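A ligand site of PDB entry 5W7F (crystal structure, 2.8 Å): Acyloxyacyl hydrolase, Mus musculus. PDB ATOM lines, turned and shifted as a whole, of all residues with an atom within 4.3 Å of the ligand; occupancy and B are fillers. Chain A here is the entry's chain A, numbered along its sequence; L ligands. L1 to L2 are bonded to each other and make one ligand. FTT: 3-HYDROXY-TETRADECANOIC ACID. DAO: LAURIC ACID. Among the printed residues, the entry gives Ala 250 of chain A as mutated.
O1 of DAO L2 lies close to OD1 of Asn 360 (3.2 Å). The backbone NH (N) of Gly 328 sits at hydrogen-bond distance from an oxygen (O3) of FTT L1, at 3.4 Å.
Residues that only touch the ligand: His 517, Phe 516, Ala 250, Asn 327, Asp 249, Ala 251, Phe 255, Val 513, Leu 262, Phe 492, Leu 411, Gly 408, Pro 445, Val 33, Ile 358 and Leu 29. Hydrophobic or aromatic side chains that line the ligand: Leu 29, Val 33, Ala 250, Ala 251, Phe 255, Leu 262, Ile 358, Leu 411, Pro 445, Phe 492, Val 513, Phe 516 and His 517. 18 residues have an atom within 4 Å of the ligand: Leu 29, Val 33, Asp 249, Ala 250, Ala 251, Phe 255, Leu 262, Asn 327, Gly 328, Ile 358, Asn 360, Gly 408, Leu 411, Pro 445, Phe 492, Val 513, Phe 516 and His 517.
The side-chain amide nitrogen of Asn 360 lies close to the backbone carbonyl oxygen of Gly 328 (3.3 Å). The side-chain carboxylate (OD1) of Asp 514 sits at hydrogen-bond distance from the backbone NH (N) of His 517 (3.0 Å). The side-chain carboxylate (OD1) of Asp 514 sits at hydrogen-bond distance from the backbone NH (N) of Phe 516, 2.9 Å away. The backbone carbonyl oxygen (O) of Ala 250 is in hydrogen-bond range of the backbone NH (N) of Phe 255. The backbone NH (N) of Ile 358 is in hydrogen-bond range of the side-chain carboxylate (OD2) of Asp 249 (3.1 Å).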
ATOM      1  N   LEU A  29      19.765   8.128  -2.999  1.00  0.00           N
ATOM      2  CA  LEU A  29      19.539   6.726  -2.691  1.00  0.00           C
ATOM      3  C   LEU A  29      19.332   5.917  -3.966  1.00  0.00           C
ATOM      4  O   LEU A  29      19.994   4.898  -4.184  1.00  0.00           O
ATOM      5  CB  LEU A  29      18.326   6.591  -1.761  1.00  0.00           C
ATOM      6  CG  LEU A  29      17.925   5.168  -1.372  1.00  0.00           C
ATOM      7  CD1 LEU A  29      19.077   4.401  -0.743  1.00  0.00           C
ATOM      8  CD2 LEU A  29      16.744   5.210  -0.422  1.00  0.00           C
ATOM      9  N   VAL A  33      21.674   2.838  -5.375  1.00  0.00           N
ATOM     10  CA  VAL A  33      21.087   1.511  -5.553  1.00  0.00           C
ATOM     11  C   VAL A  33      21.385   0.992  -6.945  1.00  0.00           C
ATOM     12  O   VAL A  33      21.799  -0.160  -7.124  1.00  0.00           O
ATOM     13  CB  VAL A  33      19.570   1.560  -5.266  1.00  0.00           C
ATOM     14  CG1 VAL A  33      18.909   0.248  -5.674  1.00  0.00           C
ATOM     15  CG2 VAL A  33      19.318   1.844  -3.800  1.00  0.00           C
ATOM     16  N   ASP A 249      -0.994   1.734   8.148  1.00  0.00           N
ATOM     17  CA  ASP A 249       0.138   2.400   7.514  1.00  0.00           C
ATOM     18  C   ASP A 249       0.806   1.444   6.515  1.00  0.00           C
ATOM     19  O   ASP A 249       0.207   0.441   6.106  1.00  0.00           O
ATOM     20  CB  ASP A 249       1.085   2.896   8.614  1.00  0.00           C
ATOM     21  CG  ASP A 249       1.352   1.841   9.673  1.00  0.00           C
ATOM     22  OD1 ASP A 249       1.207   0.637   9.368  1.00  0.00           O
ATOM     23  OD2 ASP A 249       1.722   2.234  10.812  1.00  0.00           O
ATOM     24  N   ALA A 250       2.039   1.767   6.133  1.00  0.00           N
ATOM     25  CA  ALA A 250       2.739   0.993   5.119  1.00  0.00           C
ATOM     26  C   ALA A 250       2.732  -0.497   5.457  1.00  0.00           C
ATOM     27  O   ALA A 250       2.478  -1.346   4.588  1.00  0.00           O
ATOM     28  CB  ALA A 250       4.175   1.496   4.971  1.00  0.00           C
ATOM     29  N   ALA A 251       3.000  -0.831   6.713  1.00  0.00           N
ATOM     30  CA  ALA A 251       2.957  -2.237   7.127  1.00  0.00           C
ATOM     31  C   ALA A 251       1.583  -2.833   6.883  1.00  0.00           C
ATOM     32  O   ALA A 251       1.469  -3.979   6.432  1.00  0.00           O
ATOM     33  CB  ALA A 251       3.342  -2.354   8.597  1.00  0.00           C
ATOM     34  N   PHE A 255       3.933  -3.159   2.624  1.00  0.00           N
ATOM     35  CA  PHE A 255       5.035  -2.597   1.871  1.00  0.00           C
ATOM     36  C   PHE A 255       6.128  -3.641   1.730  1.00  0.00           C
ATOM     37  O   PHE A 255       6.529  -4.279   2.706  1.00  0.00           O
ATOM     38  CB  PHE A 255       5.571  -1.349   2.588  1.00  0.00           C
ATOM     39  CG  PHE A 255       6.672  -0.638   1.859  1.00  0.00           C
ATOM     40  CD1 PHE A 255       6.409   0.479   1.092  1.00  0.00           C
ATOM     41  CD2 PHE A 255       7.981  -1.080   1.956  1.00  0.00           C
ATOM     42  CE1 PHE A 255       7.418   1.138   0.419  1.00  0.00           C
ATOM     43  CE2 PHE A 255       8.995  -0.423   1.292  1.00  0.00           C
ATOM     44  CZ  PHE A 255       8.718   0.695   0.522  1.00  0.00           C
ATOM     45  N   ILE A 257       9.584  -4.401  -0.961  1.00  0.00           N
ATOM     46  CA  ILE A 257      10.479  -4.320  -2.110  1.00  0.00           C
ATOM     47  C   ILE A 257      11.171  -5.675  -2.247  1.00  0.00           C
ATOM     48  O   ILE A 257      11.992  -6.028  -1.390  1.00  0.00           O
ATOM     49  CB  ILE A 257      11.513  -3.199  -1.945  1.00  0.00           C
ATOM     50  CG1 ILE A 257      10.815  -1.836  -1.938  1.00  0.00           C
ATOM     51  CG2 ILE A 257      12.556  -3.262  -3.062  1.00  0.00           C
ATOM     52  CD1 ILE A 257      11.712  -0.691  -1.514  1.00  0.00           C
ATOM     53  N   LEU A 262      17.547  -6.143  -6.117  1.00  0.00           N
ATOM     54  CA  LEU A 262      18.787  -5.549  -5.645  1.00  0.00           C
ATOM     55  C   LEU A 262      19.935  -6.538  -5.544  1.00  0.00           C
ATOM     56  O   LEU A 262      21.081  -6.094  -5.427  1.00  0.00           O
ATOM     57  CB  LEU A 262      18.568  -4.891  -4.272  1.00  0.00           C
ATOM     58  CG  LEU A 262      17.351  -3.965  -4.177  1.00  0.00           C
ATOM     59  CD1 LEU A 262      17.236  -3.396  -2.781  1.00  0.00           C
ATOM     60  CD2 LEU A 262      17.421  -2.852  -5.202  1.00  0.00           C
ATOM     61  N   ASN A 327       1.252   4.831   3.114  1.00  0.00           N
ATOM     62  CA  ASN A 327       2.610   4.875   3.642  1.00  0.00           C
ATOM     63  C   ASN A 327       2.819   6.162   4.433  1.00  0.00           C
ATOM     64  O   ASN A 327       2.464   7.255   3.971  1.00  0.00           O
ATOM     65  CB  ASN A 327       3.621   4.798   2.496  1.00  0.00           C
ATOM     66  CG  ASN A 327       3.542   3.479   1.733  1.00  0.00           C
ATOM     67  OD1 ASN A 327       3.224   2.430   2.313  1.00  0.00           O
ATOM     68  ND2 ASN A 327       3.831   3.513   0.444  1.00  0.00           N
ATOM     69  N   GLY A 328       3.381   6.031   5.631  1.00  0.00           N
ATOM     70  CA  GLY A 328       3.562   7.166   6.514  1.00  0.00           C
ATOM     71  C   GLY A 328       2.369   7.494   7.374  1.00  0.00           C
ATOM     72  O   GLY A 328       2.411   8.484   8.119  1.00  0.00           O
ATOM     73  N   ILE A 358       0.922   1.364  13.664  1.00  0.00           N
ATOM     74  CA  ILE A 358       1.756   0.508  14.498  1.00  0.00           C
ATOM     75  C   ILE A 358       3.182   1.064  14.638  1.00  0.00           C
ATOM     76  O   ILE A 358       4.087   0.341  15.052  1.00  0.00           O
ATOM     77  CB  ILE A 358       1.780  -0.941  13.985  1.00  0.00           C
ATOM     78  CG1 ILE A 358       2.436  -1.027  12.604  1.00  0.00           C
ATOM     79  CG2 ILE A 358       0.371  -1.498  13.920  1.00  0.00           C
ATOM     80  CD1 ILE A 358       2.874  -2.425  12.218  1.00  0.00           C
ATOM     81  N   GLY A 359       3.405   2.331  14.284  1.00  0.00           N
ATOM     82  CA  GLY A 359       4.751   2.849  14.447  1.00  0.00           C
ATOM     83  C   GLY A 359       4.982   4.312  14.133  1.00  0.00           C
ATOM     84  O   GLY A 359       5.748   4.983  14.837  1.00  0.00           O
ATOM     85  N   ASN A 360       4.339   4.832  13.084  1.00  0.00           N
ATOM     86  CA  ASN A 360       4.651   6.188  12.634  1.00  0.00           C
ATOM     87  C   ASN A 360       4.440   7.250  13.703  1.00  0.00           C
ATOM     88  O   ASN A 360       4.915   8.377  13.531  1.00  0.00           O
ATOM     89  CB  ASN A 360       3.838   6.520  11.399  1.00  0.00           C
ATOM     90  CG  ASN A 360       4.315   5.798  10.169  1.00  0.00           C
ATOM     91  OD1 ASN A 360       5.505   5.505  10.030  1.00  0.00           O
ATOM     92  ND2 ASN A 360       3.399   5.496   9.264  1.00  0.00           N
ATOM     93  N   PRO A 406       4.266  -2.379  18.404  1.00  0.00           N
ATOM     94  CA  PRO A 406       5.269  -3.377  18.789  1.00  0.00           C
ATOM     95  C   PRO A 406       6.527  -2.725  19.344  1.00  0.00           C
ATOM     96  O   PRO A 406       6.762  -1.525  19.180  1.00  0.00           O
ATOM     97  CB  PRO A 406       5.566  -4.108  17.473  1.00  0.00           C
ATOM     98  CG  PRO A 406       5.357  -3.060  16.446  1.00  0.00           C
ATOM     99  CD  PRO A 406       4.247  -2.173  16.941  1.00  0.00           C
ATOM    100  N   GLY A 408       9.954  -2.129  18.776  1.00  0.00           N
ATOM    101  CA  GLY A 408      10.815  -2.155  17.608  1.00  0.00           C
ATOM    102  C   GLY A 408      12.298  -2.267  17.887  1.00  0.00           C
ATOM    103  O   GLY A 408      13.083  -2.235  16.929  1.00  0.00           O
ATOM    104  N   LEU A 411      14.231  -4.744  15.772  1.00  0.00           N
ATOM    105  CA  LEU A 411      14.869  -4.468  14.491  1.00  0.00           C
ATOM    106  C   LEU A 411      16.389  -4.461  14.617  1.00  0.00           C
ATOM    107  O   LEU A 411      17.089  -5.220  13.938  1.00  0.00           O
ATOM    108  CB  LEU A 411      14.372  -3.141  13.922  1.00  0.00           C
ATOM    109  CG  LEU A 411      12.872  -3.015  13.621  1.00  0.00           C
ATOM    110  CD1 LEU A 411      12.562  -1.622  13.081  1.00  0.00           C
ATOM    111  CD2 LEU A 411      12.418  -4.092  12.643  1.00  0.00           C
ATOM    112  N   PHE A 434      23.523   0.408   6.767  1.00  0.00           N
ATOM    113  CA  PHE A 434      22.373   0.823   5.965  1.00  0.00           C
ATOM    114  C   PHE A 434      21.513   1.822   6.723  1.00  0.00           C
ATOM    115  O   PHE A 434      21.017   2.787   6.140  1.00  0.00           O
ATOM    116  CB  PHE A 434      21.567  -0.411   5.562  1.00  0.00           C
ATOM    117  CG  PHE A 434      20.315  -0.096   4.801  1.00  0.00           C
ATOM    118  CD1 PHE A 434      20.377   0.444   3.523  1.00  0.00           C
ATOM    119  CD2 PHE A 434      19.067  -0.369   5.338  1.00  0.00           C
ATOM    120  CE1 PHE A 434      19.236   0.735   2.816  1.00  0.00           C
ATOM    121  CE2 PHE A 434      17.917  -0.088   4.635  1.00  0.00           C
ATOM    122  CZ  PHE A 434      17.999   0.460   3.369  1.00  0.00           C
ATOM    123  N   LEU A 438      20.879   5.782   5.488  1.00  0.00           N
ATOM    124  CA  LEU A 438      19.563   6.406   5.390  1.00  0.00           C
ATOM    125  C   LEU A 438      19.445   7.588   6.353  1.00  0.00           C
ATOM    126  O   LEU A 438      18.925   8.637   5.986  1.00  0.00           O
ATOM    127  CB  LEU A 438      18.476   5.369   5.683  1.00  0.00           C
ATOM    128  CG  LEU A 438      18.261   4.242   4.678  1.00  0.00           C
ATOM    129  CD1 LEU A 438      17.076   3.392   5.120  1.00  0.00           C
ATOM    130  CD2 LEU A 438      18.043   4.766   3.260  1.00  0.00           C
ATOM    131  N   PRO A 445      13.285   5.726   7.899  1.00  0.00           N
ATOM    132  CA  PRO A 445      11.862   5.779   8.269  1.00  0.00           C
ATOM    133  C   PRO A 445      11.609   5.755   9.769  1.00  0.00           C
ATOM    134  O   PRO A 445      10.523   6.166  10.188  1.00  0.00           O
ATOM    135  CB  PRO A 445      11.283   4.527   7.594  1.00  0.00           C
ATOM    136  CG  PRO A 445      12.429   3.582   7.519  1.00  0.00           C
ATOM    137  CD  PRO A 445      13.627   4.438   7.254  1.00  0.00           C
ATOM    138  N   PHE A 492       4.897  -8.607  19.753  1.00  0.00           N
ATOM    139  CA  PHE A 492       5.758  -9.188  18.735  1.00  0.00           C
ATOM    140  C   PHE A 492       6.500 -10.404  19.276  1.00  0.00           C
ATOM    141  O   PHE A 492       6.780 -11.351  18.524  1.00  0.00           O
ATOM    142  CB  PHE A 492       6.761  -8.148  18.231  1.00  0.00           C
ATOM    143  CG  PHE A 492       7.108  -8.297  16.771  1.00  0.00           C
ATOM    144  CD1 PHE A 492       6.145  -8.111  15.787  1.00  0.00           C
ATOM    145  CD2 PHE A 492       8.401  -8.601  16.374  1.00  0.00           C
ATOM    146  CE1 PHE A 492       6.458  -8.234  14.454  1.00  0.00           C
ATOM    147  CE2 PHE A 492       8.713  -8.735  15.040  1.00  0.00           C
ATOM    148  CZ  PHE A 492       7.753  -8.552  14.078  1.00  0.00           C
ATOM    149  N   VAL A 513      14.761  -5.639   2.386  1.00  0.00           N
ATOM    150  CA  VAL A 513      15.320  -4.462   1.722  1.00  0.00           C
ATOM    151  C   VAL A 513      15.297  -3.250   2.648  1.00  0.00           C
ATOM    152  O   VAL A 513      16.275  -2.521   2.747  1.00  0.00           O
ATOM    153  CB  VAL A 513      14.574  -4.193   0.405  1.00  0.00           C
ATOM    154  CG1 VAL A 513      15.042  -2.875  -0.208  1.00  0.00           C
ATOM    155  CG2 VAL A 513      14.789  -5.340  -0.557  1.00  0.00           C
ATOM    156  N   ASP A 514      14.168  -3.011   3.314  1.00  0.00           N
ATOM    157  CA  ASP A 514      14.064  -1.838   4.192  1.00  0.00           C
ATOM    158  C   ASP A 514      14.424  -2.152   5.634  1.00  0.00           C
ATOM    159  O   ASP A 514      14.681  -1.209   6.406  1.00  0.00           O
ATOM    160  CB  ASP A 514      12.657  -1.232   4.118  1.00  0.00           C
ATOM    161  CG  ASP A 514      11.559  -2.252   4.360  1.00  0.00           C
ATOM    162  OD1 ASP A 514      11.348  -2.629   5.535  1.00  0.00           O
ATOM    163  OD2 ASP A 514      10.886  -2.649   3.381  1.00  0.00           O
ATOM    164  N   PHE A 516      12.703  -2.872   8.143  1.00  0.00           N
ATOM    165  CA  PHE A 516      11.829  -2.044   8.979  1.00  0.00           C
ATOM    166  C   PHE A 516      10.464  -2.696   9.151  1.00  0.00           C
ATOM    167  O   PHE A 516      10.065  -3.044  10.265  1.00  0.00           O
ATOM    168  CB  PHE A 516      11.696  -0.653   8.378  1.00  0.00           C
ATOM    169  CG  PHE A 516      10.796   0.274   9.163  1.00  0.00           C
ATOM    170  CD1 PHE A 516      10.702   0.177  10.540  1.00  0.00           C
ATOM    171  CD2 PHE A 516      10.052   1.242   8.519  1.00  0.00           C
ATOM    172  CE1 PHE A 516       9.875   1.030  11.250  1.00  0.00           C
ATOM    173  CE2 PHE A 516       9.227   2.096   9.216  1.00  0.00           C
ATOM    174  CZ  PHE A 516       9.133   1.989  10.591  1.00  0.00           C
ATOM    175  N   HIS A 517       9.739  -2.870   8.037  1.00  0.00           N
ATOM    176  CA  HIS A 517       8.379  -3.398   8.116  1.00  0.00           C
ATOM    177  C   HIS A 517       8.405  -4.900   8.379  1.00  0.00           C
ATOM    178  O   HIS A 517       9.354  -5.590   7.994  1.00  0.00           O
ATOM    179  CB  HIS A 517       7.630  -3.141   6.812  1.00  0.00           C
ATOM    180  CG  HIS A 517       7.743  -1.739   6.324  1.00  0.00           C
ATOM    181  ND1 HIS A 517       8.469  -1.407   5.189  1.00  0.00           N
ATOM    182  CD2 HIS A 517       7.236  -0.569   6.792  1.00  0.00           C
ATOM    183  CE1 HIS A 517       8.394  -0.103   4.986  1.00  0.00           C
ATOM    184  NE2 HIS A 517       7.656   0.420   5.934  1.00  0.00           N
ATOM    185  N   PRO A 518       7.357  -5.448   9.000  1.00  0.00           N
ATOM    186  CA  PRO A 518       7.188  -6.903   9.000  1.00  0.00           C
ATOM    187  C   PRO A 518       6.824  -7.405   7.617  1.00  0.00           C
ATOM    188  O   PRO A 518       6.145  -6.728   6.841  1.00  0.00           O
ATOM    189  CB  PRO A 518       6.049  -7.132   9.998  1.00  0.00           C
ATOM    190  CG  PRO A 518       5.954  -5.868  10.787  1.00  0.00           C
ATOM    191  CD  PRO A 518       6.366  -4.777   9.853  1.00  0.00           C
HETATM  192  C1  FTT L   1       7.076   6.360   2.704  1.00  0.00           C
HETATM  193  C2  FTT L   1       7.420   5.879   4.116  1.00  0.00           C
HETATM  194  C3  FTT L   1       7.083   4.387   4.239  1.00  0.00           C
HETATM  195  C4  FTT L   1       8.338   3.516   4.397  1.00  0.00           C
HETATM  196  C5  FTT L   1       9.390   3.850   3.331  1.00  0.00           C
HETATM  197  C6  FTT L   1      10.335   2.663   3.109  1.00  0.00           C
HETATM  198  C7  FTT L   1      11.671   2.907   3.809  1.00  0.00           C
HETATM  199  C8  FTT L   1      12.650   3.631   2.886  1.00  0.00           C
HETATM  200  C9  FTT L   1      13.829   2.712   2.523  1.00  0.00           C
HETATM  201  C10 FTT L   1      13.411   1.730   1.426  1.00  0.00           C
HETATM  202  C11 FTT L   1      14.652   1.014   0.883  1.00  0.00           C
HETATM  203  C12 FTT L   1      15.102   1.705  -0.405  1.00  0.00           C
HETATM  204  C13 FTT L   1      16.548   1.283  -0.744  1.00  0.00           C
HETATM  205  C14 FTT L   1      16.540   0.144  -1.747  1.00  0.00           C
HETATM  206  O2  FTT L   1       6.160   7.204   2.527  1.00  0.00           O
HETATM  207  O3  FTT L   1       6.269   4.212   5.377  1.00  0.00           O
HETATM  208  O1  DAO L   2       6.983   5.248   7.225  1.00  0.00           O
HETATM  209  C1  DAO L   2       6.294   4.311   6.742  1.00  0.00           C
HETATM  210  C2  DAO L   2       6.180   3.002   7.517  1.00  0.00           C
HETATM  211  C3  DAO L   2       4.856   2.887   8.269  1.00  0.00           C
HETATM  212  C4  DAO L   2       4.756   1.487   8.883  1.00  0.00           C
HETATM  213  C5  DAO L   2       5.311   1.508  10.309  1.00  0.00           C
HETATM  214  C6  DAO L   2       5.622   0.069  10.741  1.00  0.00           C
HETATM  215  C7  DAO L   2       6.494   0.054  11.990  1.00  0.00           C
HETATM  216  C8  DAO L   2       7.361  -1.201  11.933  1.00  0.00           C
HETATM  217  C9  DAO L   2       7.874  -1.588  13.330  1.00  0.00           C
HETATM  218  C10 DAO L   2       8.128  -3.097  13.323  1.00  0.00           C
HETATM  219  C11 DAO L   2       9.094  -3.473  14.444  1.00  0.00           C
HETATM  220  C12 DAO L   2       8.906  -4.953  14.785  1.00  0.00           C
